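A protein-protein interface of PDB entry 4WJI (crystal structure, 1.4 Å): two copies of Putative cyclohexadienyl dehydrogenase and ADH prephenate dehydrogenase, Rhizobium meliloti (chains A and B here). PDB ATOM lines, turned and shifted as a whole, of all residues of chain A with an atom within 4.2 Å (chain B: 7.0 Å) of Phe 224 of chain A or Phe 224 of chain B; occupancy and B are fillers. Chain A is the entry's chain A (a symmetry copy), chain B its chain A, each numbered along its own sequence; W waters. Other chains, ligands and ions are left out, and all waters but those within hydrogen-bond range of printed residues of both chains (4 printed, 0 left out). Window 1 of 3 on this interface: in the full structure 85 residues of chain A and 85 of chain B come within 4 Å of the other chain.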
ATOM      1  N   PRO A 191     -22.500  -2.533  -6.935  1.00  0.00           N
ATOM      2  CA  PRO A 191     -22.966  -3.299  -8.125  1.00  0.00           C
ATOM      3  C   PRO A 191     -24.485  -3.518  -8.135  1.00  0.00           C
ATOM      4  O   PRO A 191     -25.136  -3.333  -9.187  1.00  0.00           O
ATOM      5  CB  PRO A 191     -22.175  -4.623  -7.998  1.00  0.00           C
ATOM      6  CG  PRO A 191     -20.877  -4.179  -7.392  1.00  0.00           C
ATOM      7  CD  PRO A 191     -21.262  -3.087  -6.393  1.00  0.00           C
ATOM      8  N   ALA A 195     -27.186  -1.918 -10.836  1.00  0.00           N
ATOM      9  CA  ALA A 195     -28.073  -2.794 -11.601  1.00  0.00           C
ATOM     10  C   ALA A 195     -29.542  -2.384 -11.442  1.00  0.00           C
ATOM     11  O   ALA A 195     -30.272  -2.289 -12.419  1.00  0.00           O
ATOM     12  CB  ALA A 195     -27.897  -4.239 -11.176  1.00  0.00           C
ATOM     13  N   ILE A 198     -30.044   0.831 -13.604  1.00  0.00           N
ATOM     14  CA  ILE A 198     -30.145   0.697 -15.053  1.00  0.00           C
ATOM     15  C   ILE A 198     -31.439   0.003 -15.477  1.00  0.00           C
ATOM     16  O   ILE A 198     -32.018   0.377 -16.485  1.00  0.00           O
ATOM     17  CB  ILE A 198     -28.894   0.133 -15.669  1.00  0.00           C
ATOM     18  CG1 ILE A 198     -28.915   0.371 -17.190  1.00  0.00           C
ATOM     19  CG2 ILE A 198     -28.742  -1.294 -15.357  1.00  0.00           C
ATOM     20  CD1 ILE A 198     -27.599   0.065 -17.854  1.00  0.00           C
ATOM     21  N   VAL A 199     -31.897  -0.995 -14.703  1.00  0.00           N
ATOM     22  CA  VAL A 199     -33.132  -1.628 -15.067  1.00  0.00           C
ATOM     23  C   VAL A 199     -34.312  -0.667 -14.905  1.00  0.00           C
ATOM     24  O   VAL A 199     -35.208  -0.620 -15.771  1.00  0.00           O
ATOM     25  CB  VAL A 199     -33.327  -2.925 -14.270  1.00  0.00           C
ATOM     26  CG1 VAL A 199     -34.676  -3.538 -14.601  1.00  0.00           C
ATOM     27  CG2 VAL A 199     -32.212  -3.902 -14.571  1.00  0.00           C
ATOM     28  N   GLY A 220     -26.547  -7.602 -23.381  1.00  0.00           N
ATOM     29  CA  GLY A 220     -25.860  -7.110 -22.171  1.00  0.00           C
ATOM     30  C   GLY A 220     -26.762  -6.824 -20.985  1.00  0.00           C
ATOM     31  O   GLY A 220     -26.363  -6.932 -19.837  1.00  0.00           O
ATOM     32  N   PHE A 221     -27.999  -6.431 -21.270  1.00  0.00           N
ATOM     33  CA  PHE A 221     -28.915  -5.991 -20.252  1.00  0.00           C
ATOM     34  C   PHE A 221     -29.284  -7.131 -19.320  1.00  0.00           C
ATOM     35  O   PHE A 221     -29.431  -6.902 -18.107  1.00  0.00           O
ATOM     36  CB  PHE A 221     -30.174  -5.480 -20.936  1.00  0.00           C
ATOM     37  CG  PHE A 221     -31.144  -4.769 -20.057  1.00  0.00           C
ATOM     38  CD1 PHE A 221     -30.926  -3.480 -19.636  1.00  0.00           C
ATOM     39  CD2 PHE A 221     -32.361  -5.371 -19.767  1.00  0.00           C
ATOM     40  CE1 PHE A 221     -31.868  -2.835 -18.829  1.00  0.00           C
ATOM     41  CE2 PHE A 221     -33.303  -4.729 -19.003  1.00  0.00           C
ATOM     42  CZ  PHE A 221     -33.053  -3.475 -18.539  1.00  0.00           C
ATOM     43  N   ARG A 222     -29.431  -8.338 -19.845  1.00  0.00           N
ATOM     44  CA  ARG A 222     -29.863  -9.451 -19.030  1.00  0.00           C
ATOM     45  C   ARG A 222     -28.991  -9.672 -17.766  1.00  0.00           C
ATOM     46  O   ARG A 222     -29.544 -10.037 -16.697  1.00  0.00           O
ATOM     47  CB  ARG A 222     -30.048 -10.736 -19.831  1.00  0.00           C
ATOM     48  CG  ARG A 222     -28.742 -11.248 -20.370  1.00  0.00           C
ATOM     49  CD  ARG A 222     -28.965 -12.531 -21.187  1.00  0.00           C
ATOM     50  NE  ARG A 222     -27.727 -12.995 -21.804  1.00  0.00           N
ATOM     51  CZ  ARG A 222     -27.593 -14.179 -22.395  1.00  0.00           C
ATOM     52  NH1 ARG A 222     -28.631 -14.990 -22.483  1.00  0.00           N
ATOM     53  NH2 ARG A 222     -26.410 -14.536 -22.874  1.00  0.00           N
ATOM     54  N   ASP A 223     -27.666  -9.472 -17.871  1.00  0.00           N
ATOM     55  CA  ASP A 223     -26.794  -9.654 -16.729  1.00  0.00           C
ATOM     56  C   ASP A 223     -27.219  -8.782 -15.510  1.00  0.00           C
ATOM     57  O   ASP A 223     -27.197  -9.225 -14.334  1.00  0.00           O
ATOM     58  CB  ASP A 223     -25.367  -9.314 -17.173  1.00  0.00           C
ATOM     59  CG  ASP A 223     -24.877 -10.173 -18.380  1.00  0.00           C
ATOM     60  OD1 ASP A 223     -25.344  -9.978 -19.551  1.00  0.00           O
ATOM     61  OD2 ASP A 223     -23.986 -11.025 -18.176  1.00  0.00           O
ATOM     62  N   PHE A 224     -27.617  -7.549 -15.790  1.00  0.00           N
ATOM     63  CA  PHE A 224     -28.017  -6.613 -14.751  1.00  0.00           C
ATOM     64  C   PHE A 224     -29.408  -6.976 -14.190  1.00  0.00           C
ATOM     65  O   PHE A 224     -29.713  -6.779 -12.982  1.00  0.00           O
ATOM     66  CB  PHE A 224     -28.100  -5.197 -15.316  1.00  0.00           C
ATOM     67  CG  PHE A 224     -26.779  -4.573 -15.629  1.00  0.00           C
ATOM     68  CD1 PHE A 224     -26.108  -4.886 -16.802  1.00  0.00           C
ATOM     69  CD2 PHE A 224     -26.247  -3.621 -14.786  1.00  0.00           C
ATOM     70  CE1 PHE A 224     -24.876  -4.311 -17.084  1.00  0.00           C
ATOM     71  CE2 PHE A 224     -25.031  -2.998 -15.081  1.00  0.00           C
ATOM     72  CZ  PHE A 224     -24.344  -3.338 -16.235  1.00  0.00           C
ATOM     73  N   THR A 225     -30.290  -7.471 -15.039  1.00  0.00           N
ATOM     74  CA  THR A 225     -31.639  -7.869 -14.591  1.00  0.00           C
ATOM     75  C   THR A 225     -31.588  -8.983 -13.533  1.00  0.00           C
ATOM     76  O   THR A 225     -32.492  -9.057 -12.702  1.00  0.00           O
ATOM     77  CB  THR A 225     -32.597  -8.300 -15.740  1.00  0.00           C
ATOM     78  OG1 THR A 225     -32.149  -9.542 -16.334  1.00  0.00           O
ATOM     79  CG2 THR A 225     -32.739  -7.185 -16.772  1.00  0.00           C
ATOM     80  N   ARG A 226     -30.598  -9.874 -13.598  1.00  0.00           N
ATOM     81  CA  ARG A 226     -30.490 -10.955 -12.614  1.00  0.00           C
ATOM     82  C   ARG A 226     -30.312 -10.329 -11.204  1.00  0.00           C
ATOM     83  O   ARG A 226     -31.017 -10.695 -10.258  1.00  0.00           O
ATOM     84  CB  ARG A 226     -29.355 -11.923 -12.927  1.00  0.00           C
ATOM     85  CG  ARG A 226     -29.442 -13.180 -12.041  1.00  0.00           C
ATOM     86  CD  ARG A 226     -28.218 -14.061 -12.227  1.00  0.00           C
ATOM     87  NE  ARG A 226     -27.005 -13.453 -11.687  1.00  0.00           N
ATOM     88  CZ  ARG A 226     -26.677 -13.410 -10.396  1.00  0.00           C
ATOM     89  NH1 ARG A 226     -27.455 -13.995  -9.490  1.00  0.00           N
ATOM     90  NH2 ARG A 226     -25.586 -12.741 -10.027  1.00  0.00           N
ATOM     91  N   LEU A 227     -29.377  -9.412 -11.067  1.00  0.00           N
ATOM     92  CA  LEU A 227     -29.152  -8.795  -9.755  1.00  0.00           C
ATOM     93  C   LEU A 227     -30.387  -8.023  -9.313  1.00  0.00           C
ATOM     94  O   LEU A 227     -30.763  -8.040  -8.129  1.00  0.00           O
ATOM     95  CB  LEU A 227     -27.910  -7.916  -9.787  1.00  0.00           C
ATOM     96  CG  LEU A 227     -26.630  -8.705 -10.050  1.00  0.00           C
ATOM     97  CD1 LEU A 227     -25.467  -7.754 -10.219  1.00  0.00           C
ATOM     98  CD2 LEU A 227     -26.381  -9.707  -8.925  1.00  0.00           C
ATOM     99  N   ALA A 228     -31.000  -7.317 -10.256  1.00  0.00           N
ATOM    100  CA  ALA A 228     -32.201  -6.489  -9.943  1.00  0.00           C
ATOM    101  C   ALA A 228     -33.484  -7.296  -9.744  1.00  0.00           C
ATOM    102  O   ALA A 228     -34.574  -6.727  -9.609  1.00  0.00           O
ATOM    103  CB  ALA A 228     -32.389  -5.425 -11.009  1.00  0.00           C
ATOM    104  N   SER B 188     -27.797  -2.638 -24.647  1.00  0.00           N
ATOM    105  CA  SER B 188     -26.438  -3.148 -24.800  1.00  0.00           C
ATOM    106  C   SER B 188     -25.349  -2.136 -24.473  1.00  0.00           C
ATOM    107  O   SER B 188     -24.447  -2.417 -23.704  1.00  0.00           O
ATOM    108  CB  SER B 188     -26.251  -3.635 -26.262  1.00  0.00           C
ATOM    109  OG  SER B 188     -24.938  -4.151 -26.449  1.00  0.00           O
ATOM    110  N   LEU B 190     -25.231   1.100 -23.069  1.00  0.00           N
ATOM    111  CA  LEU B 190     -25.205   1.615 -21.699  1.00  0.00           C
ATOM    112  C   LEU B 190     -24.792   0.540 -20.705  1.00  0.00           C
ATOM    113  O   LEU B 190     -23.901   0.777 -19.875  1.00  0.00           O
ATOM    114  CB  LEU B 190     -26.525   2.295 -21.317  1.00  0.00           C
ATOM    115  CG  LEU B 190     -26.539   2.940 -19.922  1.00  0.00           C
ATOM    116  CD1 LEU B 190     -25.551   4.092 -19.875  1.00  0.00           C
ATOM    117  CD2 LEU B 190     -27.915   3.422 -19.518  1.00  0.00           C
ATOM    118  N   PRO B 191     -25.376  -0.682 -20.788  1.00  0.00           N
ATOM    119  CA  PRO B 191     -24.903  -1.731 -19.842  1.00  0.00           C
ATOM    120  C   PRO B 191     -23.382  -1.934 -19.889  1.00  0.00           C
ATOM    121  O   PRO B 191     -22.731  -2.028 -18.825  1.00  0.00           O
ATOM    122  CB  PRO B 191     -25.684  -2.980 -20.315  1.00  0.00           C
ATOM    123  CG  PRO B 191     -26.986  -2.403 -20.784  1.00  0.00           C
ATOM    124  CD  PRO B 191     -26.610  -1.083 -21.459  1.00  0.00           C
ATOM    125  N   HIS B 192     -22.783  -1.988 -21.089  1.00  0.00           N
ATOM    126  CA  HIS B 192     -21.328  -2.161 -21.157  1.00  0.00           C
ATOM    127  C   HIS B 192     -20.557  -0.969 -20.568  1.00  0.00           C
ATOM    128  O   HIS B 192     -19.572  -1.148 -19.871  1.00  0.00           O
ATOM    129  CB  HIS B 192     -20.858  -2.498 -22.582  1.00  0.00           C
ATOM    130  CG  HIS B 192     -21.126  -3.915 -22.993  1.00  0.00           C
ATOM    131  ND1 HIS B 192     -22.368  -4.379 -23.373  1.00  0.00           N
ATOM    132  CD2 HIS B 192     -20.283  -4.969 -23.100  1.00  0.00           C
ATOM    133  CE1 HIS B 192     -22.266  -5.650 -23.722  1.00  0.00           C
ATOM    134  NE2 HIS B 192     -21.014  -6.037 -23.532  1.00  0.00           N
ATOM    135  N   ILE B 193     -20.979   0.250 -20.926  1.00  0.00           N
ATOM    136  CA  ILE B 193     -20.337   1.461 -20.431  1.00  0.00           C
ATOM    137  C   ILE B 193     -20.347   1.525 -18.891  1.00  0.00           C
ATOM    138  O   ILE B 193     -19.313   1.818 -18.298  1.00  0.00           O
ATOM    139  CB  ILE B 193     -21.009   2.700 -21.022  1.00  0.00           C
ATOM    140  CG1 ILE B 193     -20.642   2.793 -22.510  1.00  0.00           C
ATOM    141  CG2 ILE B 193     -20.651   3.978 -20.262  1.00  0.00           C
ATOM    142  CD1 ILE B 193     -21.568   3.706 -23.318  1.00  0.00           C
ATOM    143  N   ILE B 194     -21.503   1.180 -18.307  1.00  0.00           N
ATOM    144  CA  ILE B 194     -21.640   1.186 -16.874  1.00  0.00           C
ATOM    145  C   ILE B 194     -20.768   0.105 -16.227  1.00  0.00           C
ATOM    146  O   ILE B 194     -20.180   0.340 -15.171  1.00  0.00           O
ATOM    147  CB  ILE B 194     -23.146   1.050 -16.483  1.00  0.00           C
ATOM    148  CG1 ILE B 194     -23.979   2.252 -16.957  1.00  0.00           C
ATOM    149  CG2 ILE B 194     -23.322   0.940 -15.017  1.00  0.00           C
ATOM    150  CD1 ILE B 194     -23.492   3.611 -16.566  1.00  0.00           C
ATOM    151  N   ALA B 195     -20.691  -1.083 -16.859  1.00  0.00           N
ATOM    152  CA  ALA B 195     -19.796  -2.123 -16.351  1.00  0.00           C
ATOM    153  C   ALA B 195     -18.330  -1.675 -16.394  1.00  0.00           C
ATOM    154  O   ALA B 195     -17.600  -1.835 -15.426  1.00  0.00           O
ATOM    155  CB  ALA B 195     -19.962  -3.406 -17.142  1.00  0.00           C
ATOM    156  N   TYR B 196     -17.899  -1.092 -17.512  1.00  0.00           N
ATOM    157  CA  TYR B 196     -16.513  -0.562 -17.574  1.00  0.00           C
ATOM    158  C   TYR B 196     -16.296   0.471 -16.456  1.00  0.00           C
ATOM    159  O   TYR B 196     -15.225   0.510 -15.822  1.00  0.00           O
ATOM    160  CB  TYR B 196     -16.245   0.092 -18.928  1.00  0.00           C
ATOM    161  CG  TYR B 196     -15.941  -0.886 -20.045  1.00  0.00           C
ATOM    162  CD1 TYR B 196     -14.798  -1.677 -19.999  1.00  0.00           C
ATOM    163  CD2 TYR B 196     -16.745  -0.958 -21.211  1.00  0.00           C
ATOM    164  CE1 TYR B 196     -14.488  -2.549 -21.023  1.00  0.00           C
ATOM    165  CE2 TYR B 196     -16.409  -1.815 -22.252  1.00  0.00           C
ATOM    166  CZ  TYR B 196     -15.283  -2.595 -22.173  1.00  0.00           C
ATOM    167  OH  TYR B 196     -14.964  -3.423 -23.258  1.00  0.00           O
ATOM    168  N   ILE B 198     -17.851   0.860 -13.459  1.00  0.00           N
ATOM    169  CA  ILE B 198     -17.748   0.348 -12.097  1.00  0.00           C
ATOM    170  C   ILE B 198     -16.448  -0.423 -11.870  1.00  0.00           C
ATOM    171  O   ILE B 198     -15.871  -0.324 -10.799  1.00  0.00           O
ATOM    172  CB  ILE B 198     -18.993  -0.368 -11.654  1.00  0.00           C
ATOM    173  CG1 ILE B 198     -18.973  -0.540 -10.123  1.00  0.00           C
ATOM    174  CG2 ILE B 198     -19.135  -1.663 -12.332  1.00  0.00           C
ATOM    175  CD1 ILE B 198     -20.286  -1.020  -9.565  1.00  0.00           C
ATOM    176  N   VAL B 199     -15.983  -1.177 -12.880  1.00  0.00           N
ATOM    177  CA  VAL B 199     -14.743  -1.874 -12.695  1.00  0.00           C
ATOM    178  C   VAL B 199     -13.571  -0.896 -12.596  1.00  0.00           C
ATOM    179  O   VAL B 199     -12.674  -1.072 -11.748  1.00  0.00           O
ATOM    180  CB  VAL B 199     -14.538  -2.914 -13.806  1.00  0.00           C
ATOM    181  CG1 VAL B 199     -13.185  -3.582 -13.647  1.00  0.00           C
ATOM    182  CG2 VAL B 199     -15.645  -3.944 -13.775  1.00  0.00           C
ATOM    183  N   GLY B 220     -21.272  -9.882  -6.260  1.00  0.00           N
ATOM    184  CA  GLY B 220     -21.965  -9.094  -7.298  1.00  0.00           C
ATOM    185  C   GLY B 220     -21.066  -8.498  -8.365  1.00  0.00           C
ATOM    186  O   GLY B 220     -21.465  -8.302  -9.502  1.00  0.00           O
ATOM    187  N   PHE B 221     -19.832  -8.185  -7.986  1.00  0.00           N
ATOM    188  CA  PHE B 221     -18.921  -7.485  -8.851  1.00  0.00           C
ATOM    189  C   PHE B 221     -18.544  -8.335 -10.050  1.00  0.00           C
ATOM    190  O   PHE B 221     -18.400  -7.793 -11.160  1.00  0.00           O
ATOM    191  CB  PHE B 221     -17.665  -7.162  -8.055  1.00  0.00           C
ATOM    192  CG  PHE B 221     -16.702  -6.237  -8.713  1.00  0.00           C
ATOM    193  CD1 PHE B 221     -16.930  -4.884  -8.780  1.00  0.00           C
ATOM    194  CD2 PHE B 221     -15.480  -6.732  -9.151  1.00  0.00           C
ATOM    195  CE1 PHE B 221     -15.993  -4.042  -9.386  1.00  0.00           C
ATOM    196  CE2 PHE B 221     -14.544  -5.903  -9.717  1.00  0.00           C
ATOM    197  CZ  PHE B 221     -14.803  -4.574  -9.834  1.00  0.00           C
ATOM    198  N   ARG B 222     -18.387  -9.636  -9.863  1.00  0.00           N
ATOM    199  CA  ARG B 222     -17.947 -10.491 -10.942  1.00  0.00           C
ATOM    200  C   ARG B 222     -18.818 -10.377 -12.221  1.00  0.00           C
ATOM    201  O   ARG B 222     -18.264 -10.444 -13.347  1.00  0.00           O
ATOM    202  CB  ARG B 222     -17.752 -11.941 -10.508  1.00  0.00           C
ATOM    203  CG  ARG B 222     -19.053 -12.587 -10.125  1.00  0.00           C
ATOM    204  CD  ARG B 222     -18.819 -14.039  -9.676  1.00  0.00           C
ATOM    205  NE  ARG B 222     -20.053 -14.659  -9.204  1.00  0.00           N
ATOM    206  CZ  ARG B 222     -20.177 -15.957  -8.948  1.00  0.00           C
ATOM    207  NH1 ARG B 222     -19.133 -16.755  -9.075  1.00  0.00           N
ATOM    208  NH2 ARG B 222     -21.356 -16.438  -8.581  1.00  0.00           N
ATOM    209  N   ASP B 223     -20.145 -10.222 -12.067  1.00  0.00           N
ATOM    210  CA  ASP B 223     -21.017 -10.103 -13.218  1.00  0.00           C
ATOM    211  C   ASP B 223     -20.600  -8.937 -14.163  1.00  0.00           C
ATOM    212  O   ASP B 223     -20.620  -9.054 -15.414  1.00  0.00           O
ATOM    213  CB  ASP B 223     -22.445  -9.904 -12.701  1.00  0.00           C
ATOM    214  CG  ASP B 223     -22.928 -11.055 -11.764  1.00  0.00           C
ATOM    215  OD1 ASP B 223     -22.461 -11.173 -10.584  1.00  0.00           O
ATOM    216  OD2 ASP B 223     -23.813 -11.829 -12.187  1.00  0.00           O
ATOM    217  N   PHE B 224     -20.212  -7.818 -13.567  1.00  0.00           N
ATOM    218  CA  PHE B 224     -19.820  -6.639 -14.321  1.00  0.00           C
ATOM    219  C   PHE B 224     -18.426  -6.829 -14.957  1.00  0.00           C
ATOM    220  O   PHE B 224     -18.124  -6.318 -16.070  1.00  0.00           O
ATOM    221  CB  PHE B 224     -19.747  -5.421 -13.402  1.00  0.00           C
ATOM    222  CG  PHE B 224     -21.072  -4.913 -12.937  1.00  0.00           C
ATOM    223  CD1 PHE B 224     -21.740  -5.530 -11.889  1.00  0.00           C
ATOM    224  CD2 PHE B 224     -21.612  -3.776 -13.499  1.00  0.00           C
ATOM    225  CE1 PHE B 224     -22.976  -5.058 -11.467  1.00  0.00           C
ATOM    226  CE2 PHE B 224     -22.833  -3.263 -13.052  1.00  0.00           C
ATOM    227  CZ  PHE B 224     -23.516  -3.900 -12.029  1.00  0.00           C
ATOM    228  N   THR B 225     -17.539  -7.525 -14.268  1.00  0.00           N
ATOM    229  CA  THR B 225     -16.188  -7.780 -14.803  1.00  0.00           C
ATOM    230  C   THR B 225     -16.231  -8.575 -16.119  1.00  0.00           C
ATOM    231  O   THR B 225     -15.327  -8.420 -16.938  1.00  0.00           O
ATOM    232  CB  THR B 225     -15.225  -8.492 -13.808  1.00  0.00           C
ATOM    233  OG1 THR B 225     -15.663  -9.849 -13.564  1.00  0.00           O
ATOM    234  CG2 THR B 225     -15.091  -7.687 -12.518  1.00  0.00           C
ATOM    235  N   ARG B 226     -17.215  -9.459 -16.292  1.00  0.00           N
ATOM    236  CA  ARG B 226     -17.315 -10.243 -17.527  1.00  0.00           C
ATOM    237  C   ARG B 226     -17.499  -9.268 -18.721  1.00  0.00           C
ATOM    238  O   ARG B 226     -16.792  -9.366 -19.729  1.00  0.00           O
ATOM    239  CB  ARG B 226     -18.442 -11.268 -17.481  1.00  0.00           C
ATOM    240  CG  ARG B 226     -18.346 -12.245 -18.668  1.00  0.00           C
ATOM    241  CD  ARG B 226     -19.564 -13.154 -18.723  1.00  0.00           C
ATOM    242  NE  ARG B 226     -20.782 -12.434 -19.084  1.00  0.00           N
ATOM    243  CZ  ARG B 226     -21.112 -12.054 -20.318  1.00  0.00           C
ATOM    244  NH1 ARG B 226     -20.329 -12.373 -21.346  1.00  0.00           N
ATOM    245  NH2 ARG B 226     -22.208 -11.320 -20.499  1.00  0.00           N
ATOM    246  N   LEU B 227     -18.442  -8.355 -18.612  1.00  0.00           N
ATOM    247  CA  LEU B 227     -18.673  -7.415 -19.715  1.00  0.00           C
ATOM    248  C   LEU B 227     -17.445  -6.544 -19.936  1.00  0.00           C
ATOM    249  O   LEU B 227     -17.070  -6.245 -21.082  1.00  0.00           O
ATOM    250  CB  LEU B 227     -19.922  -6.585 -19.454  1.00  0.00           C
ATOM    251  CG  LEU B 227     -21.195  -7.425 -19.409  1.00  0.00           C
ATOM    252  CD1 LEU B 227     -22.366  -6.562 -18.997  1.00  0.00           C
ATOM    253  CD2 LEU B 227     -21.437  -8.096 -20.759  1.00  0.00           C
ATOM    254  N   ALA B 228     -16.836  -6.107 -18.839  1.00  0.00           N
ATOM    255  CA  ALA B 228     -15.641  -5.217 -18.922  1.00  0.00           C
ATOM    256  C   ALA B 228     -14.352  -5.932 -19.325  1.00  0.00           C
ATOM    257  O   ALA B 228     -13.267  -5.340 -19.304  1.00  0.00           O
ATOM    258  CB  ALA B 228     -15.461  -4.471 -17.612  1.00  0.00           C
ATOM    259  N   ALA B 229     -14.466  -7.208 -19.680  1.00  0.00           N
ATOM    260  CA  ALA B 229     -13.362  -7.956 -20.296  1.00  0.00           C
ATOM    261  C   ALA B 229     -13.422  -8.080 -21.820  1.00  0.00           C
ATOM    262  O   ALA B 229     -12.540  -8.726 -22.436  1.00  0.00           O
ATOM    263  CB  ALA B 229     -13.285  -9.336 -19.703  1.00  0.00           C
ATOM    264  N   PHE B 253     -29.937   7.747 -17.233  1.00  0.00           N
ATOM    265  CA  PHE B 253     -29.344   6.926 -16.177  1.00  0.00           C
ATOM    266  C   PHE B 253     -28.841   7.791 -15.021  1.00  0.00           C
ATOM    267  O   PHE B 253     -29.086   7.474 -13.858  1.00  0.00           O
ATOM    268  CB  PHE B 253     -28.185   6.087 -16.761  1.00  0.00           C
ATOM    269  CG  PHE B 253     -27.388   5.346 -15.718  1.00  0.00           C
ATOM    270  CD1 PHE B 253     -26.321   5.963 -15.078  1.00  0.00           C
ATOM    271  CD2 PHE B 253     -27.709   4.037 -15.354  1.00  0.00           C
ATOM    272  CE1 PHE B 253     -25.617   5.333 -14.074  1.00  0.00           C
ATOM    273  CE2 PHE B 253     -26.979   3.389 -14.364  1.00  0.00           C
ATOM    274  CZ  PHE B 253     -25.935   4.034 -13.730  1.00  0.00           C
ATOM    275  N   ARG B 283     -37.109  -9.020 -15.111  1.00  0.00           N
ATOM    276  CA  ARG B 283     -36.366 -10.277 -15.076  1.00  0.00           C
ATOM    277  C   ARG B 283     -37.298 -11.450 -15.327  1.00  0.00           C
ATOM    278  O   ARG B 283     -36.995 -12.408 -16.049  1.00  0.00           O
ATOM    279  CB  ARG B 283     -35.695 -10.489 -13.709  1.00  0.00           C
ATOM    280  CG  ARG B 283     -34.967 -11.828 -13.642  1.00  0.00           C
ATOM    281  CD  ARG B 283     -33.843 -11.925 -14.631  1.00  0.00           C
ATOM    282  NE  ARG B 283     -33.092 -13.158 -14.485  1.00  0.00           N
ATOM    283  CZ  ARG B 283     -31.976 -13.420 -15.172  1.00  0.00           C
ATOM    284  NH1 ARG B 283     -31.503 -12.517 -16.047  1.00  0.00           N
ATOM    285  NH2 ARG B 283     -31.337 -14.562 -14.997  1.00  0.00           N
HETATM  286  O   HOH W   1     -24.775 -13.423 -19.586  1.00  0.00           O
HETATM  287  O   HOH W   2     -21.923 -11.194 -16.557  1.00  0.00           O
HETATM  288  O   HOH W   3     -23.003 -14.509 -11.460  1.00  0.00           O
HETATM  289  O   HOH W   4     -25.876 -11.581 -13.796  1.00  0.00           O
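Of the printed residues of chain B, Phe 224 of chain A touches Pro 191 (3.3 Å), Phe 224 (3.0 Å) and Leu 227 (3.9 Å).
Of the printed residues of chain A, Phe 224 of chain B touches Pro 191 (3.3 Å), Phe 224 (3.0 Å) and Leu 227 (3.9 Å).
Printed residues of chain B within 4 Å of Leu 227 of chain A: Phe 224 (3.9 Å).
Printed residues of chain A within 4 Å of Arg 226 of chain B: Asp 223.
Printed residues of chain A within 4 Å of Arg 283 of chain B: Arg 222 (3.2 Å), Thr 225 (3.1 Å) and Arg 226 (3.7 Å).
Printed residues of chain B within 4 Å of Arg 226 of chain A: Asp 223 (2.9 Å) and Arg 283 (3.7 Å).
Of the printed residues of chain A, Phe 253 of chain B touches Ile 198 (3.996 Å).
The nearest printed residue of chain B that does not touch Leu 227 of chain A is Gly 220 of chain B (4.1 Å).
The side-chain carboxylate (OD2) of Asp 223 of chain B is in salt-bridge range of the guanidinium group (NH2) of Arg 226 of chain A (2.9 Å).
OD2 of Asp 223 of chain A is in salt-bridge range of NH2 of Arg 226 of chain B (2.9 Å).
The backbone carbonyl oxygen (O) of Arg 222 of chain A sits at hydrogen-bond distance from the guanidinium group (NH1) of Arg 283 of chain B, at 3.2 Å.
NH1 of Arg 283 of chain B sits at hydrogen-bond distance from OG1 of Thr 225 of chain A (3.1 Å).
Pro 191 of chain A touches Ile 198 of chain B, and with the chains exchanged Ile 198 of chain A touches Pro 191 of chain B.
Asp 223 of chain A touches Arg 226 of chain B, and with the chains exchanged Arg 226 of chain A touches Asp 223 of chain B.
Phe 224 of chain B touches its own counterpart, Phe 224 of chain A.
Phe 224 of chain A touches Leu 227 of chain B, and with the chains exchanged Leu 227 of chain A touches Phe 224 of chain B.
Of the 22 printed residues of chain B, 9 touch a printed residue of chain A.
Of the 13 printed residues of chain A, 8 touch a printed residue of chain B.
Hydrophobic or aromatic side chains of chain A that line the printed part of chain B: Pro 191, Ile 198, Phe 224 and Leu 227.
O of Arg 222 of chain A lies within hydrogen-bond range of OG1 of Thr 225 of chain A, 2.7 Å away.
CD1 of Ile 198 of chain B touches N of Pro 191 of chain A, 3.8 Å away.
O of Pro 191 of chain A touches CZ of Phe 224 of chain B (3.3 Å).
Ile 198 of chain A touches Leu 190 of chain B.
Pro 191 of chain B touches Ile 198 of chain A.
CE2 of Phe 253 of chain B touches CB of Ile 198 of chain A (3.996 Å).
Phe 224 of chain A touches Pro 191 of chain B.
Phe 224 of chain B touches Phe 224 of chain A (CE2 to CE2, 3.0 Å).
CE1 of Phe 224 of chain A touches CD1 of Leu 227 of chain B (3.9 Å).
Arg 283 of chain B touches Arg 226 of chain A.
Leu 227 of chain A touches Phe 224 of chain B.
Water W4 lies within hydrogen-bond range of OD2 of Asp 223 of chain B (2.6 Å), O of Asp 223 of chain A (2.8 Å) and NE of Arg 226 of chain A (3.0 Å).
Water W2 lies within hydrogen-bond range of the side-chain carboxylate of Asp 223 of chain A (2.6 Å), the backbone carbonyl oxygen of Asp 223 of chain B (2.8 Å) and the guanidinium group of Arg 226 of chain B (3.0 Å).
Water W1 bridges the side-chain carboxylate of Asp 223 of chain A (2.9 Å) and the guanidinium group of Arg 226 of chain B (3.4 Å).
Water W3 bridges the side-chain carboxylate (OD2) of Asp 223 of chain B (2.9 Å) and the guanidinium group (NH2) of Arg 226 of chain A (3.4 Å).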
